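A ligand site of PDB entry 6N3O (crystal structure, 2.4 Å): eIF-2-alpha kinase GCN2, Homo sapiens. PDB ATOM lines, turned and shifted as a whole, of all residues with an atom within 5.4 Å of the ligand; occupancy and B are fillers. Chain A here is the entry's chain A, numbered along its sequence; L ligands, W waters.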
ATOM      1  N   LEU A  23      28.122  18.254 -31.660  1.00  0.00           N
ATOM      2  CA  LEU A  23      26.814  17.617 -31.374  1.00  0.00           C
ATOM      3  C   LEU A  23      26.218  18.199 -30.085  1.00  0.00           C
ATOM      4  O   LEU A  23      24.998  18.134 -29.928  1.00  0.00           O
ATOM      5  CB  LEU A  23      26.998  16.112 -31.262  1.00  0.00           C
ATOM      6  CG  LEU A  23      27.540  15.408 -32.496  1.00  0.00           C
ATOM      7  CD1 LEU A  23      27.705  13.910 -32.254  1.00  0.00           C
ATOM      8  CD2 LEU A  23      26.647  15.643 -33.711  1.00  0.00           C
ATOM      9  N   VAL A  31      30.649  17.033 -27.078  1.00  0.00           N
ATOM     10  CA  VAL A  31      30.542  15.860 -27.989  1.00  0.00           C
ATOM     11  C   VAL A  31      30.726  16.336 -29.431  1.00  0.00           C
ATOM     12  O   VAL A  31      29.933  17.184 -29.896  1.00  0.00           O
ATOM     13  CB  VAL A  31      29.209  15.108 -27.817  1.00  0.00           C
ATOM     14  CG1 VAL A  31      29.210  13.817 -28.606  1.00  0.00           C
ATOM     15  CG2 VAL A  31      28.928  14.842 -26.346  1.00  0.00           C
ATOM     16  N   ALA A  44      30.937   9.530 -32.454  1.00  0.00           N
ATOM     17  CA  ALA A  44      30.770  10.663 -31.514  1.00  0.00           C
ATOM     18  C   ALA A  44      31.868  10.550 -30.453  1.00  0.00           C
ATOM     19  O   ALA A  44      31.958   9.505 -29.822  1.00  0.00           O
ATOM     20  CB  ALA A  44      29.403  10.636 -30.890  1.00  0.00           C
ATOM     21  N   VAL A  45      32.685  11.589 -30.298  1.00  0.00           N
ATOM     22  CA  VAL A  45      33.769  11.604 -29.293  1.00  0.00           C
ATOM     23  C   VAL A  45      33.457  12.716 -28.280  1.00  0.00           C
ATOM     24  O   VAL A  45      33.322  13.876 -28.707  1.00  0.00           O
ATOM     25  CB  VAL A  45      35.149  11.774 -29.950  1.00  0.00           C
ATOM     26  CG1 VAL A  45      36.235  11.934 -28.894  1.00  0.00           C
ATOM     27  CG2 VAL A  45      35.476  10.621 -30.872  1.00  0.00           C
ATOM     28  N   LYS A  46      33.307  12.341 -27.012  1.00  0.00           N
ATOM     29  CA  LYS A  46      33.185  13.271 -25.873  1.00  0.00           C
ATOM     30  C   LYS A  46      34.595  13.593 -25.392  1.00  0.00           C
ATOM     31  O   LYS A  46      35.417  12.672 -25.276  1.00  0.00           O
ATOM     32  CB  LYS A  46      32.317  12.683 -24.765  1.00  0.00           C
ATOM     33  CG  LYS A  46      31.879  13.669 -23.691  1.00  0.00           C
ATOM     34  CD  LYS A  46      31.108  13.049 -22.549  1.00  0.00           C
ATOM     35  CE  LYS A  46      29.800  12.405 -22.946  1.00  0.00           C
ATOM     36  NZ  LYS A  46      28.628  13.200 -22.526  1.00  0.00           N
ATOM     37  N   GLU A  63      33.343   5.156 -13.531  1.00  0.00           N
ATOM     38  CA  GLU A  63      32.118   5.118 -14.359  1.00  0.00           C
ATOM     39  C   GLU A  63      32.511   4.627 -15.757  1.00  0.00           C
ATOM     40  O   GLU A  63      31.712   3.877 -16.355  1.00  0.00           O
ATOM     41  CB  GLU A  63      31.404   6.467 -14.271  1.00  0.00           C
ATOM     42  CG  GLU A  63      30.904   6.782 -12.859  1.00  0.00           C
ATOM     43  CD  GLU A  63      30.040   5.724 -12.189  1.00  0.00           C
ATOM     44  OE1 GLU A  63      29.173   5.145 -12.877  1.00  0.00           O
ATOM     45  OE2 GLU A  63      30.218   5.488 -10.958  1.00  0.00           O
ATOM     46  N   VAL A  64      33.720   4.920 -16.214  1.00  0.00           N
ATOM     47  CA  VAL A  64      34.202   4.431 -17.548  1.00  0.00           C
ATOM     48  C   VAL A  64      34.361   2.903 -17.481  1.00  0.00           C
ATOM     49  O   VAL A  64      33.906   2.247 -18.445  1.00  0.00           O
ATOM     50  CB  VAL A  64      35.507   5.084 -18.006  1.00  0.00           C
ATOM     51  CG1 VAL A  64      36.106   4.362 -19.210  1.00  0.00           C
ATOM     52  CG2 VAL A  64      35.329   6.568 -18.314  1.00  0.00           C
ATOM     53  N   LEU A  67      30.646   1.493 -17.372  1.00  0.00           N
ATOM     54  CA  LEU A  67      29.790   1.666 -18.578  1.00  0.00           C
ATOM     55  C   LEU A  67      30.417   0.924 -19.770  1.00  0.00           C
ATOM     56  O   LEU A  67      29.643   0.466 -20.622  1.00  0.00           O
ATOM     57  CB  LEU A  67      29.619   3.149 -18.897  1.00  0.00           C
ATOM     58  CG  LEU A  67      29.006   3.997 -17.791  1.00  0.00           C
ATOM     59  CD1 LEU A  67      29.143   5.477 -18.103  1.00  0.00           C
ATOM     60  CD2 LEU A  67      27.544   3.629 -17.589  1.00  0.00           C
ATOM     61  N   SER A  68      31.749   0.772 -19.803  1.00  0.00           N
ATOM     62  CA  SER A  68      32.464  -0.009 -20.848  1.00  0.00           C
ATOM     63  C   SER A  68      31.953  -1.452 -20.903  1.00  0.00           C
ATOM     64  O   SER A  68      32.113  -2.065 -21.954  1.00  0.00           O
ATOM     65  CB  SER A  68      33.954   0.020 -20.680  1.00  0.00           C
ATOM     66  OG  SER A  68      34.337  -0.644 -19.500  1.00  0.00           O
ATOM     67  N   LEU A  70      28.750  -2.476 -20.625  1.00  0.00           N
ATOM     68  CA  LEU A  70      27.352  -2.569 -21.146  1.00  0.00           C
ATOM     69  C   LEU A  70      27.350  -3.012 -22.623  1.00  0.00           C
ATOM     70  O   LEU A  70      28.126  -2.451 -23.405  1.00  0.00           O
ATOM     71  CB  LEU A  70      26.666  -1.207 -20.983  1.00  0.00           C
ATOM     72  CG  LEU A  70      26.383  -0.795 -19.537  1.00  0.00           C
ATOM     73  CD1 LEU A  70      25.839   0.627 -19.498  1.00  0.00           C
ATOM     74  CD2 LEU A  70      25.391  -1.749 -18.864  1.00  0.00           C
ATOM     75  N   ILE A  75      21.641   0.282 -26.239  1.00  0.00           N
ATOM     76  CA  ILE A  75      22.651   1.179 -25.601  1.00  0.00           C
ATOM     77  C   ILE A  75      23.577   1.714 -26.689  1.00  0.00           C
ATOM     78  O   ILE A  75      24.014   0.931 -27.537  1.00  0.00           O
ATOM     79  CB  ILE A  75      23.473   0.442 -24.521  1.00  0.00           C
ATOM     80  CG1 ILE A  75      22.582  -0.298 -23.527  1.00  0.00           C
ATOM     81  CG2 ILE A  75      24.422   1.412 -23.824  1.00  0.00           C
ATOM     82  CD1 ILE A  75      21.851   0.588 -22.586  1.00  0.00           C
ATOM     83  N   VAL A  76      23.902   2.993 -26.672  1.00  0.00           N
ATOM     84  CA  VAL A  76      24.916   3.524 -27.604  1.00  0.00           C
ATOM     85  C   VAL A  76      26.161   2.640 -27.440  1.00  0.00           C
ATOM     86  O   VAL A  76      26.603   2.441 -26.311  1.00  0.00           O
ATOM     87  CB  VAL A  76      25.202   5.014 -27.344  1.00  0.00           C
ATOM     88  CG1 VAL A  76      26.244   5.571 -28.313  1.00  0.00           C
ATOM     89  CG2 VAL A  76      23.928   5.826 -27.421  1.00  0.00           C
ATOM     90  N   TYR A  78      29.997   1.391 -27.404  1.00  0.00           N
ATOM     91  CA  TYR A  78      31.265   1.977 -26.905  1.00  0.00           C
ATOM     92  C   TYR A  78      32.430   1.434 -27.743  1.00  0.00           C
ATOM     93  O   TYR A  78      32.460   0.265 -28.072  1.00  0.00           O
ATOM     94  CB  TYR A  78      31.433   1.678 -25.408  1.00  0.00           C
ATOM     95  CG  TYR A  78      32.826   1.824 -24.840  1.00  0.00           C
ATOM     96  CD1 TYR A  78      33.339   3.049 -24.451  1.00  0.00           C
ATOM     97  CD2 TYR A  78      33.638   0.720 -24.681  1.00  0.00           C
ATOM     98  CE1 TYR A  78      34.620   3.169 -23.940  1.00  0.00           C
ATOM     99  CE2 TYR A  78      34.910   0.818 -24.155  1.00  0.00           C
ATOM    100  CZ  TYR A  78      35.408   2.045 -23.784  1.00  0.00           C
ATOM    101  OH  TYR A  78      36.670   2.100 -23.248  1.00  0.00           O
ATOM    102  N   ALA A  81      38.227   4.652 -24.947  1.00  0.00           N
ATOM    103  CA  ALA A  81      38.467   5.742 -23.980  1.00  0.00           C
ATOM    104  C   ALA A  81      39.974   5.898 -23.840  1.00  0.00           C
ATOM    105  O   ALA A  81      40.666   4.891 -23.891  1.00  0.00           O
ATOM    106  CB  ALA A  81      37.804   5.403 -22.676  1.00  0.00           C
ATOM    107  N   ILE A 104      36.156   9.889 -25.068  1.00  0.00           N
ATOM    108  CA  ILE A 104      35.309   8.670 -25.136  1.00  0.00           C
ATOM    109  C   ILE A 104      34.707   8.632 -26.535  1.00  0.00           C
ATOM    110  O   ILE A 104      33.952   9.542 -26.902  1.00  0.00           O
ATOM    111  CB  ILE A 104      34.268   8.665 -24.008  1.00  0.00           C
ATOM    112  CG1 ILE A 104      34.953   8.830 -22.656  1.00  0.00           C
ATOM    113  CG2 ILE A 104      33.398   7.426 -24.028  1.00  0.00           C
ATOM    114  CD1 ILE A 104      33.998   9.104 -21.572  1.00  0.00           C
ATOM    115  N   MET A 106      32.300   6.831 -29.089  1.00  0.00           N
ATOM    116  CA  MET A 106      31.044   6.028 -29.181  1.00  0.00           C
ATOM    117  C   MET A 106      30.558   5.987 -30.625  1.00  0.00           C
ATOM    118  O   MET A 106      31.078   6.710 -31.468  1.00  0.00           O
ATOM    119  CB  MET A 106      29.942   6.639 -28.340  1.00  0.00           C
ATOM    120  CG  MET A 106      30.374   6.996 -26.926  1.00  0.00           C
ATOM    121  SD  MET A 106      30.728   5.553 -25.883  1.00  0.00           S
ATOM    122  CE  MET A 106      29.112   4.786 -25.768  1.00  0.00           C
ATOM    123  N   GLU A 107      29.584   5.114 -30.873  1.00  0.00           N
ATOM    124  CA  GLU A 107      28.742   5.066 -32.091  1.00  0.00           C
ATOM    125  C   GLU A 107      28.179   6.466 -32.339  1.00  0.00           C
ATOM    126  O   GLU A 107      27.812   7.139 -31.352  1.00  0.00           O
ATOM    127  CB  GLU A 107      27.665   4.006 -31.900  1.00  0.00           C
ATOM    128  CG  GLU A 107      26.396   4.196 -32.710  1.00  0.00           C
ATOM    129  CD  GLU A 107      25.321   3.140 -32.435  1.00  0.00           C
ATOM    130  OE1 GLU A 107      24.449   2.941 -33.317  1.00  0.00           O
ATOM    131  OE2 GLU A 107      25.352   2.521 -31.339  1.00  0.00           O
ATOM    132  N   TYR A 108      28.195   6.908 -33.584  1.00  0.00           N
ATOM    133  CA  TYR A 108      27.407   8.077 -34.051  1.00  0.00           C
ATOM    134  C   TYR A 108      26.047   7.565 -34.519  1.00  0.00           C
ATOM    135  O   TYR A 108      26.012   6.709 -35.389  1.00  0.00           O
ATOM    136  CB  TYR A 108      28.138   8.822 -35.163  1.00  0.00           C
ATOM    137  CG  TYR A 108      27.279   9.871 -35.813  1.00  0.00           C
ATOM    138  CD1 TYR A 108      26.758  10.907 -35.062  1.00  0.00           C
ATOM    139  CD2 TYR A 108      26.938   9.790 -37.159  1.00  0.00           C
ATOM    140  CE1 TYR A 108      25.935  11.856 -35.630  1.00  0.00           C
ATOM    141  CE2 TYR A 108      26.123  10.737 -37.739  1.00  0.00           C
ATOM    142  CZ  TYR A 108      25.623  11.779 -36.967  1.00  0.00           C
ATOM    143  OH  TYR A 108      24.820  12.737 -37.524  1.00  0.00           O
ATOM    144  N   CYS A 109      24.960   8.082 -33.948  1.00  0.00           N
ATOM    145  CA  CYS A 109      23.569   7.705 -34.290  1.00  0.00           C
ATOM    146  C   CYS A 109      23.013   8.688 -35.338  1.00  0.00           C
ATOM    147  O   CYS A 109      22.892   9.895 -35.031  1.00  0.00           O
ATOM    148  CB  CYS A 109      22.738   7.669 -33.017  1.00  0.00           C
ATOM    149  SG  CYS A 109      23.454   6.546 -31.786  1.00  0.00           S
ATOM    150  N   GLU A 110      22.736   8.186 -36.530  1.00  0.00           N
ATOM    151  CA  GLU A 110      22.536   9.010 -37.757  1.00  0.00           C
ATOM    152  C   GLU A 110      21.243   9.839 -37.638  1.00  0.00           C
ATOM    153  O   GLU A 110      21.241  10.952 -38.176  1.00  0.00           O
ATOM    154  CB  GLU A 110      22.561   8.129 -39.006  1.00  0.00           C
ATOM    155  CG  GLU A 110      23.908   7.420 -39.222  1.00  0.00           C
ATOM    156  CD  GLU A 110      24.077   6.006 -38.663  1.00  0.00           C
ATOM    157  OE1 GLU A 110      23.682   5.718 -37.478  1.00  0.00           O
ATOM    158  OE2 GLU A 110      24.626   5.171 -39.423  1.00  0.00           O
ATOM    159  N   SER A 112      19.841  11.279 -35.020  1.00  0.00           N
ATOM    160  CA  SER A 112      19.857  12.291 -33.937  1.00  0.00           C
ATOM    161  C   SER A 112      19.162  11.763 -32.662  1.00  0.00           C
ATOM    162  O   SER A 112      19.257  10.565 -32.389  1.00  0.00           O
ATOM    163  CB  SER A 112      19.251  13.569 -34.434  1.00  0.00           C
ATOM    164  OG  SER A 112      19.436  14.612 -33.486  1.00  0.00           O
ATOM    165  N   PHE A 159      19.180   8.417 -28.258  1.00  0.00           N
ATOM    166  CA  PHE A 159      19.593   8.634 -29.663  1.00  0.00           C
ATOM    167  C   PHE A 159      18.858   7.632 -30.550  1.00  0.00           C
ATOM    168  O   PHE A 159      18.271   6.671 -30.018  1.00  0.00           O
ATOM    169  CB  PHE A 159      21.107   8.559 -29.799  1.00  0.00           C
ATOM    170  CG  PHE A 159      21.825   9.517 -28.882  1.00  0.00           C
ATOM    171  CD1 PHE A 159      21.940  10.857 -29.200  1.00  0.00           C
ATOM    172  CD2 PHE A 159      22.355   9.079 -27.674  1.00  0.00           C
ATOM    173  CE1 PHE A 159      22.588  11.741 -28.348  1.00  0.00           C
ATOM    174  CE2 PHE A 159      22.986   9.973 -26.817  1.00  0.00           C
ATOM    175  CZ  PHE A 159      23.096  11.297 -27.161  1.00  0.00           C
ATOM    176  N   ILE A 168      20.288   4.283 -25.935  1.00  0.00           N
ATOM    177  CA  ILE A 168      20.403   5.104 -24.698  1.00  0.00           C
ATOM    178  C   ILE A 168      21.881   5.412 -24.458  1.00  0.00           C
ATOM    179  O   ILE A 168      22.720   4.523 -24.648  1.00  0.00           O
ATOM    180  CB  ILE A 168      19.740   4.415 -23.494  1.00  0.00           C
ATOM    181  CG1 ILE A 168      18.256   4.152 -23.762  1.00  0.00           C
ATOM    182  CG2 ILE A 168      19.943   5.236 -22.235  1.00  0.00           C
ATOM    183  CD1 ILE A 168      17.682   3.014 -22.948  1.00  0.00           C
ATOM    184  N   GLY A 169      22.188   6.642 -24.055  1.00  0.00           N
ATOM    185  CA  GLY A 169      23.553   7.068 -23.696  1.00  0.00           C
ATOM    186  C   GLY A 169      23.522   8.215 -22.715  1.00  0.00           C
ATOM    187  O   GLY A 169      22.450   8.508 -22.147  1.00  0.00           O
ATOM    188  N   ASP A 170      24.675   8.840 -22.505  1.00  0.00           N
ATOM    189  CA  ASP A 170      24.850  10.029 -21.640  1.00  0.00           C
ATOM    190  C   ASP A 170      24.361   9.681 -20.242  1.00  0.00           C
ATOM    191  O   ASP A 170      23.516  10.415 -19.708  1.00  0.00           O
ATOM    192  CB  ASP A 170      24.115  11.227 -22.230  1.00  0.00           C
ATOM    193  CG  ASP A 170      24.920  11.950 -23.283  1.00  0.00           C
ATOM    194  OD1 ASP A 170      26.166  11.953 -23.178  1.00  0.00           O
ATOM    195  OD2 ASP A 170      24.287  12.519 -24.190  1.00  0.00           O
ATOM    196  N   PHE A 171      24.907   8.615 -19.666  1.00  0.00           N
ATOM    197  CA  PHE A 171      24.726   8.214 -18.244  1.00  0.00           C
ATOM    198  C   PHE A 171      25.175   9.385 -17.372  1.00  0.00           C
ATOM    199  O   PHE A 171      24.488   9.711 -16.408  1.00  0.00           O
ATOM    200  CB  PHE A 171      25.503   6.924 -17.958  1.00  0.00           C
ATOM    201  CG  PHE A 171      24.800   5.705 -18.492  1.00  0.00           C
ATOM    202  CD1 PHE A 171      24.733   5.470 -19.859  1.00  0.00           C
ATOM    203  CD2 PHE A 171      24.169   4.819 -17.630  1.00  0.00           C
ATOM    204  CE1 PHE A 171      24.068   4.363 -20.355  1.00  0.00           C
ATOM    205  CE2 PHE A 171      23.504   3.712 -18.126  1.00  0.00           C
ATOM    206  CZ  PHE A 171      23.460   3.474 -19.486  1.00  0.00           C
ATOM    207  N   GLY A 172      26.282  10.024 -17.750  1.00  0.00           N
ATOM    208  CA  GLY A 172      26.925  11.064 -16.936  1.00  0.00           C
ATOM    209  C   GLY A 172      28.055  10.451 -16.149  1.00  0.00           C
ATOM    210  O   GLY A 172      27.786   9.642 -15.242  1.00  0.00           O
ATOM    211  N   LEU A 173      29.276  10.828 -16.478  1.00  0.00           N
ATOM    212  CA  LEU A 173      30.492  10.192 -15.937  1.00  0.00           C
ATOM    213  C   LEU A 173      30.797  10.674 -14.514  1.00  0.00           C
ATOM    214  O   LEU A 173      31.647  10.045 -13.898  1.00  0.00           O
ATOM    215  CB  LEU A 173      31.632  10.482 -16.899  1.00  0.00           C
ATOM    216  CG  LEU A 173      31.399   9.845 -18.259  1.00  0.00           C
ATOM    217  CD1 LEU A 173      32.451  10.280 -19.244  1.00  0.00           C
ATOM    218  CD2 LEU A 173      31.379   8.337 -18.156  1.00  0.00           C
HETATM  219  C1  LIG L   1      30.371   9.812 -25.270  1.00  0.00           C
HETATM  220  C2  LIG L   1      30.484   6.230 -21.592  1.00  0.00           C
HETATM  221  C3  LIG L   1      25.424  12.026 -29.792  1.00  0.00           C
HETATM  222  C4  LIG L   1      25.787   9.917 -30.719  1.00  0.00           C
HETATM  223  C5  LIG L   1      30.389   3.934 -22.167  1.00  0.00           C
HETATM  224  C6  LIG L   1      28.264   9.883 -26.440  1.00  0.00           C
HETATM  225  C7  LIG L   1      27.681   9.265 -25.350  1.00  0.00           C
HETATM  226  C8  LIG L   1      31.119   5.008 -21.709  1.00  0.00           C
HETATM  227  C9  LIG L   1      24.552  11.479 -31.820  1.00  0.00           C
HETATM  228  C10 LIG L   1      26.765  10.418 -28.507  1.00  0.00           C
HETATM  229  C11 LIG L   1      27.450  10.192 -27.560  1.00  0.00           C
HETATM  230  C12 LIG L   1      29.782   9.189 -24.191  1.00  0.00           C
HETATM  231  C13 LIG L   1      25.994  10.781 -29.668  1.00  0.00           C
HETATM  232  C14 LIG L   1      28.432   8.918 -24.256  1.00  0.00           C
HETATM  233  C15 LIG L   1      29.608  10.148 -26.387  1.00  0.00           C
HETATM  234  C16 LIG L   1      29.143   6.277 -21.933  1.00  0.00           C
HETATM  235  C17 LIG L   1      28.481   5.143 -22.363  1.00  0.00           C
HETATM  236  C18 LIG L   1      26.617   4.044 -23.206  1.00  0.00           C
HETATM  237  N1  LIG L   1      29.084   3.957 -22.498  1.00  0.00           N
HETATM  238  N2  LIG L   1      24.701  12.385 -30.854  1.00  0.00           N
HETATM  239  N3  LIG L   1      25.074  10.237 -31.794  1.00  0.00           N
HETATM  240  N4  LIG L   1      23.816  11.822 -32.938  1.00  0.00           N
HETATM  241  N5  LIG L   1      27.649   8.268 -23.269  1.00  0.00           N
HETATM  242  O1  LIG L   1      29.229   8.799 -21.208  1.00  0.00           O
HETATM  243  O2  LIG L   1      27.098   7.518 -21.007  1.00  0.00           O
HETATM  244  O3  LIG L   1      27.149   5.273 -22.671  1.00  0.00           O
HETATM  245  F1  LIG L   1      30.169  10.745 -27.428  1.00  0.00           F
HETATM  246  F2  LIG L   1      26.381   8.984 -25.341  1.00  0.00           F
HETATM  247  S1  LIG L   1      28.283   7.832 -21.769  1.00  0.00           S
HETATM  248 CL1  LIG L   1      32.801   4.835 -21.326  1.00  0.00          CL
HETATM  249  O   HOH W   1      27.852  10.820 -20.006  1.00  0.00           O
HETATM  250  O   HOH W   2      22.543  14.536 -33.661  1.00  0.00           O
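O2 of the ligand lies within hydrogen-bond range of N of Phe 171 (2.8 Å).
O of Cys 109 lies within hydrogen-bond range of N4 of the ligand (3.0 Å).
The backbone NH (N) of Asp 170 is in hydrogen-bond range of an oxygen (O2) of the ligand, 3.1 Å away.
N3 of the ligand lies within hydrogen-bond range of N of Cys 109, at 3.0 Å.
N of Ala 81 lies within hydrogen-bond range of OH of Tyr 78 (3.4 Å).
The backbone NH (N) of Lys 46 is in hydrogen-bond range of the backbone carbonyl oxygen (O) of Ile 104 (2.9 Å).
The side-chain hydroxyl (OG) of Ser 68 lies within hydrogen-bond range of the backbone carbonyl oxygen (O) of Val 64 (3.1 Å).
The backbone NH (N) of Met 106 lies within hydrogen-bond range of the backbone carbonyl oxygen (O) of Ala 44, at 2.8 Å.
The backbone NH (N) of Leu 23 lies within hydrogen-bond range of the backbone carbonyl oxygen (O) of Val 31 (2.7 Å).
The backbone NH of Val 76 sits at hydrogen-bond distance from the backbone carbonyl oxygen of Ile 168 (2.8 Å).
The side-chain amino group (NZ) of Lys 46 lies within salt-bridge range of the side-chain carboxylate (OD1) of Asp 170, at 2.8 Å.
The backbone carbonyl oxygen (O) of Ala 44 sits close to a fluorine (F1) of the ligand.
Leu 23 touches the ligand (CD1 to N2, 3.6 Å).
Val 31 touches the ligand (CG1 to F1, 3.4 Å).
N of Val 45 touches F1 of the ligand, at 3.9 Å.
Lys 46 touches the ligand.
CG1 of Val 64 touches CL1 of the ligand (3.95 Å).
Leu 67 touches the ligand.
CG2 of Ile 75 touches C18 of the ligand (3.5 Å).
Val 76 touches the ligand (O to C18, 3.5 Å).
CE1 of Tyr 78 touches CL1 of the ligand (3.6 Å).
Ile 104 touches the ligand.
Met 106 touches the ligand (CG to C1, 3.3 Å).
O of Glu 107 touches C4 of the ligand, 3.5 Å away.
Tyr 108 touches the ligand.
CE1 of Phe 159 touches C3 of the ligand (3.2 Å).
Gly 169 touches the ligand (CA to F2, 3.8 Å).
CD2 of Leu 173 touches O1 of the ligand (3.8 Å).
Hydrophobic or aromatic side chains that line the ligand: Leu 23, Val 31, Ala 44, Val 64, Leu 67, Ile 75, Tyr 78, Ile 104, Met 106, Tyr 108, Phe 159, Phe 171 and Leu 173.
Of the 28 residues printed, 20 come within 4 Å of the ligand.
The nearest printed residue that does not touch the ligand is Ser 112 (4.1 Å).
Water W1 lies within hydrogen-bond range of an oxygen (O1) of the ligand (2.7 Å) and the backbone NH of Gly 172 (2.9 Å).
Water W2 bridges N4 of the ligand and OG of Ser 112.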
